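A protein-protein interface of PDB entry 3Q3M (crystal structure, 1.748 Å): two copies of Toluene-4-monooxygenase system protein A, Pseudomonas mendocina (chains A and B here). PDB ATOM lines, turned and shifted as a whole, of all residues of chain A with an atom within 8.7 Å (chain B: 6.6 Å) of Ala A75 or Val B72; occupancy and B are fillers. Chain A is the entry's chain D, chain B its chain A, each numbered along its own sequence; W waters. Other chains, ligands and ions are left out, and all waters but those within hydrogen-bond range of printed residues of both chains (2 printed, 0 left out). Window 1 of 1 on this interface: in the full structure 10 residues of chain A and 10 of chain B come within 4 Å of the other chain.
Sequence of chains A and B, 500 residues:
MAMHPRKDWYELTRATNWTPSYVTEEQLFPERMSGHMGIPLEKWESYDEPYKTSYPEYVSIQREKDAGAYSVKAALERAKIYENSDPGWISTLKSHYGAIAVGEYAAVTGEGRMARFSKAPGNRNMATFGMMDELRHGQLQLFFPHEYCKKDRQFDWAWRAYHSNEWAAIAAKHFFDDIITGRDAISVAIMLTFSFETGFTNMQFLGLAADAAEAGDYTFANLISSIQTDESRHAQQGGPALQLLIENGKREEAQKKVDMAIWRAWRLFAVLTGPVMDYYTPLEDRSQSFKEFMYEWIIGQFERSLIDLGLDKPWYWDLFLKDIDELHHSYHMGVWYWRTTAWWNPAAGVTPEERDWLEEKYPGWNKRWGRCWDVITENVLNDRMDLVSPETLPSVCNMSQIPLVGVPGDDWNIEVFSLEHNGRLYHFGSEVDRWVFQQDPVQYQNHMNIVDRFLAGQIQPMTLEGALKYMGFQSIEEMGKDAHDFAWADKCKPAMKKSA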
ATOM      1  N   ALA A  67     -29.139  21.203  35.475  1.00  0.00           N
ATOM      2  CA  ALA A  67     -27.712  20.930  35.643  1.00  0.00           C
ATOM      3  C   ALA A  67     -26.967  21.128  34.323  1.00  0.00           C
ATOM      4  O   ALA A  67     -25.917  21.764  34.295  1.00  0.00           O
ATOM      5  CB  ALA A  67     -27.471  19.516  36.198  1.00  0.00           C
ATOM      6  N   GLY A  68     -27.537  20.625  33.233  1.00  0.00           N
ATOM      7  CA  GLY A  68     -26.937  20.805  31.924  1.00  0.00           C
ATOM      8  C   GLY A  68     -26.925  22.268  31.481  1.00  0.00           C
ATOM      9  O   GLY A  68     -25.893  22.773  31.030  1.00  0.00           O
ATOM     10  N   ALA A  69     -28.046  22.969  31.622  1.00  0.00           N
ATOM     11  CA  ALA A  69     -28.110  24.360  31.156  1.00  0.00           C
ATOM     12  C   ALA A  69     -27.065  25.207  31.876  1.00  0.00           C
ATOM     13  O   ALA A  69     -26.384  26.019  31.271  1.00  0.00           O
ATOM     14  CB  ALA A  69     -29.495  24.935  31.398  1.00  0.00           C
ATOM     15  N   TYR A  70     -26.941  25.020  33.180  1.00  0.00           N
ATOM     16  CA  TYR A  70     -25.995  25.834  33.944  1.00  0.00           C
ATOM     17  C   TYR A  70     -24.519  25.446  33.728  1.00  0.00           C
ATOM     18  O   TYR A  70     -23.639  26.315  33.731  1.00  0.00           O
ATOM     19  CB  TYR A  70     -26.333  25.833  35.431  1.00  0.00           C
ATOM     20  CG  TYR A  70     -27.568  26.626  35.804  1.00  0.00           C
ATOM     21  CD1 TYR A  70     -27.536  28.015  35.880  1.00  0.00           C
ATOM     22  CD2 TYR A  70     -28.764  25.990  36.076  1.00  0.00           C
ATOM     23  CE1 TYR A  70     -28.687  28.756  36.245  1.00  0.00           C
ATOM     24  CE2 TYR A  70     -29.924  26.720  36.428  1.00  0.00           C
ATOM     25  CZ  TYR A  70     -29.880  28.087  36.504  1.00  0.00           C
ATOM     26  OH  TYR A  70     -31.022  28.796  36.842  1.00  0.00           O
ATOM     27  N   SER A  71     -24.252  24.155  33.549  1.00  0.00           N
ATOM     28  CA  SER A  71     -22.872  23.712  33.304  1.00  0.00           C
ATOM     29  C   SER A  71     -22.370  24.308  31.998  1.00  0.00           C
ATOM     30  O   SER A  71     -21.217  24.742  31.886  1.00  0.00           O
ATOM     31  CB  SER A  71     -22.783  22.188  33.200  1.00  0.00           C
ATOM     32  OG  SER A  71     -23.018  21.571  34.434  1.00  0.00           O
ATOM     33  N   VAL A  72     -23.233  24.291  30.991  1.00  0.00           N
ATOM     34  CA  VAL A  72     -22.848  24.799  29.687  1.00  0.00           C
ATOM     35  C   VAL A  72     -22.533  26.287  29.797  1.00  0.00           C
ATOM     36  O   VAL A  72     -21.484  26.755  29.314  1.00  0.00           O
ATOM     37  CB  VAL A  72     -23.934  24.527  28.608  1.00  0.00           C
ATOM     38  CG1 VAL A  72     -23.602  25.274  27.324  1.00  0.00           C
ATOM     39  CG2 VAL A  72     -24.053  23.015  28.340  1.00  0.00           C
ATOM     40  N   LYS A  73     -23.415  27.046  30.452  1.00  0.00           N
ATOM     41  CA  LYS A  73     -23.143  28.468  30.689  1.00  0.00           C
ATOM     42  C   LYS A  73     -21.778  28.631  31.365  1.00  0.00           C
ATOM     43  O   LYS A  73     -20.939  29.425  30.943  1.00  0.00           O
ATOM     44  CB  LYS A  73     -24.240  29.084  31.581  1.00  0.00           C
ATOM     45  CG  LYS A  73     -24.007  30.570  31.892  1.00  0.00           C
ATOM     46  CD  LYS A  73     -25.114  31.066  32.870  1.00  0.00           C
ATOM     47  CE  LYS A  73     -24.971  32.568  33.136  1.00  0.00           C
ATOM     48  NZ  LYS A  73     -23.691  32.922  33.882  1.00  0.00           N
ATOM     49  N   ALA A  74     -21.534  27.855  32.415  1.00  0.00           N
ATOM     50  CA  ALA A  74     -20.283  28.014  33.153  1.00  0.00           C
ATOM     51  C   ALA A  74     -19.049  27.719  32.302  1.00  0.00           C
ATOM     52  O   ALA A  74     -18.034  28.403  32.410  1.00  0.00           O
ATOM     53  CB  ALA A  74     -20.305  27.136  34.406  1.00  0.00           C
ATOM     54  N   ALA A  75     -19.137  26.694  31.458  1.00  0.00           N
ATOM     55  CA  ALA A  75     -17.965  26.224  30.714  1.00  0.00           C
ATOM     56  C   ALA A  75     -17.628  27.192  29.592  1.00  0.00           C
ATOM     57  O   ALA A  75     -16.515  27.213  29.109  1.00  0.00           O
ATOM     58  CB  ALA A  75     -18.243  24.837  30.159  1.00  0.00           C
ATOM     59  N   LEU A  76     -18.599  28.013  29.209  1.00  0.00           N
ATOM     60  CA  LEU A  76     -18.389  28.956  28.106  1.00  0.00           C
ATOM     61  C   LEU A  76     -18.289  30.431  28.514  1.00  0.00           C
ATOM     62  O   LEU A  76     -18.297  31.301  27.652  1.00  0.00           O
ATOM     63  CB  LEU A  76     -19.494  28.791  27.056  1.00  0.00           C
ATOM     64  CG  LEU A  76     -19.625  27.398  26.437  1.00  0.00           C
ATOM     65  CD1 LEU A  76     -20.823  27.371  25.473  1.00  0.00           C
ATOM     66  CD2 LEU A  76     -18.340  26.991  25.701  1.00  0.00           C
ATOM     67  N   GLU A  77     -18.165  30.730  29.801  1.00  0.00           N
ATOM     68  CA  GLU A  77     -18.120  32.141  30.175  1.00  0.00           C
ATOM     69  C   GLU A  77     -17.001  32.893  29.472  1.00  0.00           C
ATOM     70  O   GLU A  77     -17.124  34.105  29.260  1.00  0.00           O
ATOM     71  CB  GLU A  77     -17.984  32.321  31.677  1.00  0.00           C
ATOM     72  CG  GLU A  77     -19.120  31.767  32.449  1.00  0.00           C
ATOM     73  CD  GLU A  77     -20.358  32.633  32.351  1.00  0.00           C
ATOM     74  OE1 GLU A  77     -21.301  32.372  33.104  1.00  0.00           O
ATOM     75  OE2 GLU A  77     -20.392  33.569  31.526  1.00  0.00           O
ATOM     76  N   ARG A  78     -15.917  32.199  29.104  1.00  0.00           N
ATOM     77  CA  ARG A  78     -14.755  32.868  28.495  1.00  0.00           C
ATOM     78  C   ARG A  78     -14.704  32.795  26.963  1.00  0.00           C
ATOM     79  O   ARG A  78     -13.686  33.137  26.340  1.00  0.00           O
ATOM     80  CB  ARG A  78     -13.431  32.334  29.086  1.00  0.00           C
ATOM     81  CG  ARG A  78     -13.379  32.285  30.633  1.00  0.00           C
ATOM     82  CD  ARG A  78     -13.589  33.655  31.272  1.00  0.00           C
ATOM     83  NE  ARG A  78     -12.678  34.662  30.720  1.00  0.00           N
ATOM     84  CZ  ARG A  78     -11.379  34.751  31.021  1.00  0.00           C
ATOM     85  NH1 ARG A  78     -10.822  33.902  31.896  1.00  0.00           N
ATOM     86  NH2 ARG A  78     -10.633  35.685  30.438  1.00  0.00           N
ATOM     87  N   ALA A  79     -15.798  32.372  26.352  1.00  0.00           N
ATOM     88  CA  ALA A  79     -15.873  32.275  24.896  1.00  0.00           C
ATOM     89  C   ALA A  79     -15.903  33.653  24.188  1.00  0.00           C
ATOM     90  O   ALA A  79     -15.844  33.726  22.955  1.00  0.00           O
ATOM     91  CB  ALA A  79     -17.084  31.441  24.493  1.00  0.00           C
ATOM     92  N   LYS A  80     -16.000  34.722  24.982  1.00  0.00           N
ATOM     93  CA  LYS A  80     -16.028  36.113  24.505  1.00  0.00           C
ATOM     94  C   LYS A  80     -17.201  36.442  23.600  1.00  0.00           C
ATOM     95  O   LYS A  80     -17.072  37.238  22.676  1.00  0.00           O
ATOM     96  CB  LYS A  80     -14.711  36.514  23.818  1.00  0.00           C
ATOM     97  CG  LYS A  80     -13.562  36.750  24.792  1.00  0.00           C
ATOM     98  CD  LYS A  80     -12.422  37.520  24.133  1.00  0.00           C
ATOM     99  CE  LYS A  80     -11.182  37.519  25.016  1.00  0.00           C
ATOM    100  NZ  LYS A  80     -11.478  37.907  26.433  1.00  0.00           N
ATOM    101  N   TYR A 218     -23.551  28.984  21.907  1.00  0.00           N
ATOM    102  CA  TYR A 218     -24.155  27.730  22.374  1.00  0.00           C
ATOM    103  C   TYR A 218     -24.757  27.842  23.750  1.00  0.00           C
ATOM    104  O   TYR A 218     -25.690  27.108  24.072  1.00  0.00           O
ATOM    105  CB  TYR A 218     -23.181  26.543  22.254  1.00  0.00           C
ATOM    106  CG  TYR A 218     -22.754  26.377  20.832  1.00  0.00           C
ATOM    107  CD1 TYR A 218     -23.574  25.725  19.917  1.00  0.00           C
ATOM    108  CD2 TYR A 218     -21.554  26.909  20.380  1.00  0.00           C
ATOM    109  CE1 TYR A 218     -23.201  25.606  18.579  1.00  0.00           C
ATOM    110  CE2 TYR A 218     -21.169  26.779  19.048  1.00  0.00           C
ATOM    111  CZ  TYR A 218     -22.001  26.128  18.155  1.00  0.00           C
ATOM    112  OH  TYR A 218     -21.625  26.014  16.823  1.00  0.00           O
ATOM    113  N   THR A 219     -24.277  28.793  24.549  1.00  0.00           N
ATOM    114  CA  THR A 219     -24.892  29.009  25.859  1.00  0.00           C
ATOM    115  C   THR A 219     -26.374  29.349  25.658  1.00  0.00           C
ATOM    116  O   THR A 219     -27.266  28.765  26.298  1.00  0.00           O
ATOM    117  CB  THR A 219     -24.199  30.134  26.630  1.00  0.00           C
ATOM    118  OG1 THR A 219     -22.868  29.698  26.972  1.00  0.00           O
ATOM    119  CG2 THR A 219     -24.985  30.452  27.925  1.00  0.00           C
ATOM    120  N   ASN A 222     -28.435  26.432  23.648  1.00  0.00           N
ATOM    121  CA  ASN A 222     -28.698  25.320  24.552  1.00  0.00           C
ATOM    122  C   ASN A 222     -29.769  25.676  25.602  1.00  0.00           C
ATOM    123  O   ASN A 222     -30.638  24.857  25.909  1.00  0.00           O
ATOM    124  CB  ASN A 222     -27.392  24.881  25.232  1.00  0.00           C
ATOM    125  CG  ASN A 222     -27.577  23.618  26.052  1.00  0.00           C
ATOM    126  OD1 ASN A 222     -27.882  22.560  25.498  1.00  0.00           O
ATOM    127  ND2 ASN A 222     -27.426  23.724  27.357  1.00  0.00           N
ATOM    128  N   ALA B  67     -21.561  14.911  35.263  1.00  0.00           N
ATOM    129  CA  ALA B  67     -22.735  15.472  34.581  1.00  0.00           C
ATOM    130  C   ALA B  67     -22.350  16.700  33.770  1.00  0.00           C
ATOM    131  O   ALA B  67     -22.814  16.873  32.649  1.00  0.00           O
ATOM    132  CB  ALA B  67     -23.815  15.848  35.576  1.00  0.00           C
ATOM    133  N   GLY B  68     -21.511  17.560  34.352  1.00  0.00           N
ATOM    134  CA  GLY B  68     -21.035  18.747  33.653  1.00  0.00           C
ATOM    135  C   GLY B  68     -20.186  18.386  32.430  1.00  0.00           C
ATOM    136  O   GLY B  68     -20.372  18.957  31.352  1.00  0.00           O
ATOM    137  N   ALA B  69     -19.253  17.456  32.586  1.00  0.00           N
ATOM    138  CA  ALA B  69     -18.343  17.127  31.480  1.00  0.00           C
ATOM    139  C   ALA B  69     -19.118  16.595  30.284  1.00  0.00           C
ATOM    140  O   ALA B  69     -18.845  16.961  29.134  1.00  0.00           O
ATOM    141  CB  ALA B  69     -17.332  16.106  31.905  1.00  0.00           C
ATOM    142  N   TYR B  70     -20.050  15.677  30.544  1.00  0.00           N
ATOM    143  CA  TYR B  70     -20.852  15.123  29.467  1.00  0.00           C
ATOM    144  C   TYR B  70     -21.861  16.114  28.872  1.00  0.00           C
ATOM    145  O   TYR B  70     -22.116  16.103  27.666  1.00  0.00           O
ATOM    146  CB  TYR B  70     -21.569  13.824  29.913  1.00  0.00           C
ATOM    147  CG  TYR B  70     -20.625  12.653  30.129  1.00  0.00           C
ATOM    148  CD1 TYR B  70     -20.152  11.904  29.053  1.00  0.00           C
ATOM    149  CD2 TYR B  70     -20.202  12.293  31.413  1.00  0.00           C
ATOM    150  CE1 TYR B  70     -19.292  10.816  29.265  1.00  0.00           C
ATOM    151  CE2 TYR B  70     -19.333  11.217  31.631  1.00  0.00           C
ATOM    152  CZ  TYR B  70     -18.888  10.474  30.554  1.00  0.00           C
ATOM    153  OH  TYR B  70     -18.012   9.424  30.741  1.00  0.00           O
ATOM    154  N   SER B  71     -22.455  16.961  29.708  1.00  0.00           N
ATOM    155  CA  SER B  71     -23.410  17.937  29.181  1.00  0.00           C
ATOM    156  C   SER B  71     -22.718  18.903  28.221  1.00  0.00           C
ATOM    157  O   SER B  71     -23.238  19.255  27.155  1.00  0.00           O
ATOM    158  CB  SER B  71     -24.050  18.747  30.314  1.00  0.00           C
ATOM    159  OG  SER B  71     -24.984  17.963  31.002  1.00  0.00           O
ATOM    160  N   VAL B  72     -21.536  19.344  28.620  1.00  0.00           N
ATOM    161  CA  VAL B  72     -20.773  20.249  27.776  1.00  0.00           C
ATOM    162  C   VAL B  72     -20.441  19.588  26.448  1.00  0.00           C
ATOM    163  O   VAL B  72     -20.632  20.181  25.380  1.00  0.00           O
ATOM    164  CB  VAL B  72     -19.502  20.779  28.521  1.00  0.00           C
ATOM    165  CG1 VAL B  72     -18.578  21.543  27.550  1.00  0.00           C
ATOM    166  CG2 VAL B  72     -19.965  21.669  29.662  1.00  0.00           C
ATOM    167  N   LYS B  73     -19.954  18.354  26.493  1.00  0.00           N
ATOM    168  CA  LYS B  73     -19.688  17.629  25.255  1.00  0.00           C
ATOM    169  C   LYS B  73     -20.943  17.583  24.384  1.00  0.00           C
ATOM    170  O   LYS B  73     -20.906  17.885  23.184  1.00  0.00           O
ATOM    171  CB  LYS B  73     -19.190  16.219  25.574  1.00  0.00           C
ATOM    172  CG  LYS B  73     -18.946  15.323  24.326  1.00  0.00           C
ATOM    173  CD  LYS B  73     -18.678  13.867  24.789  1.00  0.00           C
ATOM    174  CE  LYS B  73     -18.292  12.946  23.613  1.00  0.00           C
ATOM    175  NZ  LYS B  73     -19.418  12.759  22.626  1.00  0.00           N
ATOM    176  N   ALA B  74     -22.073  17.204  24.978  1.00  0.00           N
ATOM    177  CA  ALA B  74     -23.291  17.044  24.198  1.00  0.00           C
ATOM    178  C   ALA B  74     -23.731  18.375  23.572  1.00  0.00           C
ATOM    179  O   ALA B  74     -24.192  18.399  22.430  1.00  0.00           O
ATOM    180  CB  ALA B  74     -24.408  16.469  25.082  1.00  0.00           C
ATOM    181  N   ALA B  75     -23.599  19.486  24.313  1.00  0.00           N
ATOM    182  CA  ALA B  75     -24.083  20.776  23.822  1.00  0.00           C
ATOM    183  C   ALA B  75     -23.216  21.356  22.702  1.00  0.00           C
ATOM    184  O   ALA B  75     -23.675  22.237  21.963  1.00  0.00           O
ATOM    185  CB  ALA B  75     -24.192  21.799  24.982  1.00  0.00           C
ATOM    186  N   LEU B  76     -21.971  20.880  22.593  1.00  0.00           N
ATOM    187  CA  LEU B  76     -21.036  21.398  21.593  1.00  0.00           C
ATOM    188  C   LEU B  76     -20.742  20.460  20.427  1.00  0.00           C
ATOM    189  O   LEU B  76     -19.867  20.766  19.627  1.00  0.00           O
ATOM    190  CB  LEU B  76     -19.701  21.789  22.249  1.00  0.00           C
ATOM    191  CG  LEU B  76     -19.846  22.877  23.306  1.00  0.00           C
ATOM    192  CD1 LEU B  76     -18.490  23.129  24.010  1.00  0.00           C
ATOM    193  CD2 LEU B  76     -20.408  24.142  22.685  1.00  0.00           C
ATOM    194  N   GLU B  77     -21.455  19.342  20.316  1.00  0.00           N
ATOM    195  CA  GLU B  77     -21.193  18.398  19.223  1.00  0.00           C
ATOM    196  C   GLU B  77     -21.206  19.074  17.857  1.00  0.00           C
ATOM    197  O   GLU B  77     -20.487  18.643  16.962  1.00  0.00           O
ATOM    198  CB  GLU B  77     -22.214  17.268  19.199  1.00  0.00           C
ATOM    199  CG  GLU B  77     -22.218  16.395  20.431  1.00  0.00           C
ATOM    200  CD  GLU B  77     -20.986  15.532  20.539  1.00  0.00           C
ATOM    201  OE1 GLU B  77     -20.904  14.735  21.499  1.00  0.00           O
ATOM    202  OE2 GLU B  77     -20.104  15.633  19.656  1.00  0.00           O
ATOM    203  N   PHE B 144     -14.796  10.164  24.903  1.00  0.00           N
ATOM    204  CA  PHE B 144     -14.748  11.438  24.218  1.00  0.00           C
ATOM    205  C   PHE B 144     -14.221  11.320  22.777  1.00  0.00           C
ATOM    206  O   PHE B 144     -14.888  11.804  21.867  1.00  0.00           O
ATOM    207  CB  PHE B 144     -14.014  12.512  25.034  1.00  0.00           C
ATOM    208  CG  PHE B 144     -14.917  13.251  25.998  1.00  0.00           C
ATOM    209  CD1 PHE B 144     -15.629  12.561  26.986  1.00  0.00           C
ATOM    210  CD2 PHE B 144     -15.009  14.629  25.953  1.00  0.00           C
ATOM    211  CE1 PHE B 144     -16.439  13.238  27.879  1.00  0.00           C
ATOM    212  CE2 PHE B 144     -15.822  15.317  26.853  1.00  0.00           C
ATOM    213  CZ  PHE B 144     -16.545  14.624  27.805  1.00  0.00           C
ATOM    214  N   TYR B 218     -13.796  24.079  23.785  1.00  0.00           N
ATOM    215  CA  TYR B 218     -14.193  24.053  25.190  1.00  0.00           C
ATOM    216  C   TYR B 218     -14.566  22.665  25.656  1.00  0.00           C
ATOM    217  O   TYR B 218     -14.436  22.351  26.831  1.00  0.00           O
ATOM    218  CB  TYR B 218     -15.304  25.084  25.482  1.00  0.00           C
ATOM    219  CG  TYR B 218     -14.783  26.469  25.197  1.00  0.00           C
ATOM    220  CD1 TYR B 218     -13.892  27.079  26.075  1.00  0.00           C
ATOM    221  CD2 TYR B 218     -15.125  27.139  24.027  1.00  0.00           C
ATOM    222  CE1 TYR B 218     -13.368  28.357  25.802  1.00  0.00           C
ATOM    223  CE2 TYR B 218     -14.599  28.410  23.745  1.00  0.00           C
ATOM    224  CZ  TYR B 218     -13.731  29.008  24.643  1.00  0.00           C
ATOM    225  OH  TYR B 218     -13.220  30.271  24.366  1.00  0.00           O
ATOM    226  N   THR B 219     -15.000  21.802  24.750  1.00  0.00           N
ATOM    227  CA  THR B 219     -15.310  20.431  25.196  1.00  0.00           C
ATOM    228  C   THR B 219     -14.056  19.811  25.790  1.00  0.00           C
ATOM    229  O   THR B 219     -14.089  19.205  26.872  1.00  0.00           O
ATOM    230  CB  THR B 219     -15.800  19.556  24.024  1.00  0.00           C
ATOM    231  OG1 THR B 219     -17.103  20.008  23.625  1.00  0.00           O
ATOM    232  CG2 THR B 219     -15.899  18.063  24.435  1.00  0.00           C
ATOM    233  N   PHE B 220     -12.943  19.972  25.084  1.00  0.00           N
ATOM    234  CA  PHE B 220     -11.654  19.425  25.538  1.00  0.00           C
ATOM    235  C   PHE B 220     -11.089  20.149  26.770  1.00  0.00           C
ATOM    236  O   PHE B 220     -10.684  19.506  27.742  1.00  0.00           O
ATOM    237  CB  PHE B 220     -10.642  19.460  24.373  1.00  0.00           C
ATOM    238  CG  PHE B 220      -9.346  18.730  24.650  1.00  0.00           C
ATOM    239  CD1 PHE B 220      -9.331  17.366  24.856  1.00  0.00           C
ATOM    240  CD2 PHE B 220      -8.154  19.415  24.658  1.00  0.00           C
ATOM    241  CE1 PHE B 220      -8.132  16.670  25.080  1.00  0.00           C
ATOM    242  CE2 PHE B 220      -6.941  18.728  24.903  1.00  0.00           C
ATOM    243  CZ  PHE B 220      -6.943  17.347  25.104  1.00  0.00           C
ATOM    244  N   ASN B 222     -12.611  21.878  28.985  1.00  0.00           N
ATOM    245  CA  ASN B 222     -13.465  21.557  30.130  1.00  0.00           C
ATOM    246  C   ASN B 222     -13.255  20.140  30.642  1.00  0.00           C
ATOM    247  O   ASN B 222     -13.190  19.908  31.867  1.00  0.00           O
ATOM    248  CB  ASN B 222     -14.950  21.809  29.786  1.00  0.00           C
ATOM    249  CG  ASN B 222     -15.841  21.682  31.004  1.00  0.00           C
ATOM    250  OD1 ASN B 222     -15.750  22.500  31.925  1.00  0.00           O
ATOM    251  ND2 ASN B 222     -16.688  20.659  31.023  1.00  0.00           N
ATOM    252  N   LEU B 223     -13.103  19.190  29.719  1.00  0.00           N
ATOM    253  CA  LEU B 223     -12.830  17.815  30.117  1.00  0.00           C
ATOM    254  C   LEU B 223     -11.534  17.674  30.911  1.00  0.00           C
ATOM    255  O   LEU B 223     -11.512  17.099  32.014  1.00  0.00           O
ATOM    256  CB  LEU B 223     -12.744  16.889  28.880  1.00  0.00           C
ATOM    257  CG  LEU B 223     -12.189  15.488  29.165  1.00  0.00           C
ATOM    258  CD1 LEU B 223     -13.198  14.660  29.945  1.00  0.00           C
ATOM    259  CD2 LEU B 223     -11.828  14.797  27.854  1.00  0.00           C
HETATM  260  O   HOH W   1     -11.513  33.160  24.284  1.00  0.00           O
HETATM  261  O   HOH W   2     -24.732  18.719  34.226  1.00  0.00           O
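OG of Ser B71 is in hydrogen-bond range of O of Ala B67 (2.9 Å). OG of Ser A71 is in hydrogen-bond range of O of Ala A67, at 2.9 Å.
Among the printed residues, pairs that only touch across the chains: Gly A68 with Ser B71, Ser A71 with Gly B68, Ser A71 with Val B72, Val A72 with Ala B75, Ala A75 with Val B72, Ala A75 with Asn B222, Leu A76 with Tyr B218, Arg A78 with Tyr B218, Ala A79 with Tyr B218, Tyr A218 with Leu B76 and Asn A222 with Ala B75.
Of the printed residues of chain B, Gly A68 touches Ser B71. Printed residues of chain B within 4 Å of Ala A75: Val B72 (3.6 Å) and Asn B222 (3.8 Å). Glu A77 touches none of the printed residues of chain B. Printed residues of chain B within 4 Å of Asn A222: Ala B75. Printed residues of chain A within 4 Å of Gly B68: Ser A71. Of the printed residues of chain A, Val B72 touches Ser A71 (3.99 Å) and Ala A75 (3.6 Å). The nearest printed residue of chain B that does not touch Ala A75 is Tyr B218 (4.01 Å).
Of the 17 printed residues of chain A, 9 touch a printed residue of chain B. Printed residues of chain B that touch a printed residue of chain A: Gly B68, Ser B71, Val B72, Ala B75, Leu B76, Tyr B218 and Asn B222. Hydrophobic or aromatic side chains of chain B that line the printed part of chain A: Val B72, Ala B75, Leu B76 and Tyr B218.
Gly A68 touches Ser B71, and with the chains exchanged Ser A71 touches Gly B68. Ser A71 touches Val B72, but with the chains exchanged Val A72 does not touch Ser B71 (4.03 Å). Val A72 touches Ala B75, and with the chains exchanged Ala A75 touches Val B72. Ala A75 touches Asn B222, and with the chains exchanged Asn A222 touches Ala B75. Of the 11 pairs that touch across the chains among the printed residues, 8 have their exchanged pair printed and touching as well.
Water W1 lies within hydrogen-bond range of the backbone carbonyl oxygen (O) of Arg A78 (3.0 Å) and the side-chain hydroxyl (OH) of Tyr B218 (3.4 Å). Water W2 lies within hydrogen-bond range of the backbone carbonyl oxygen of Ala B67 (3.1 Å), the backbone carbonyl oxygen of Ala A67 (3.3 Å), the side-chain hydroxyl of Ser B71 (3.3 Å), the side-chain hydroxyl of Ser A71 (3.3 Å) and the backbone NH of Gly B68 (3.4 Å).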
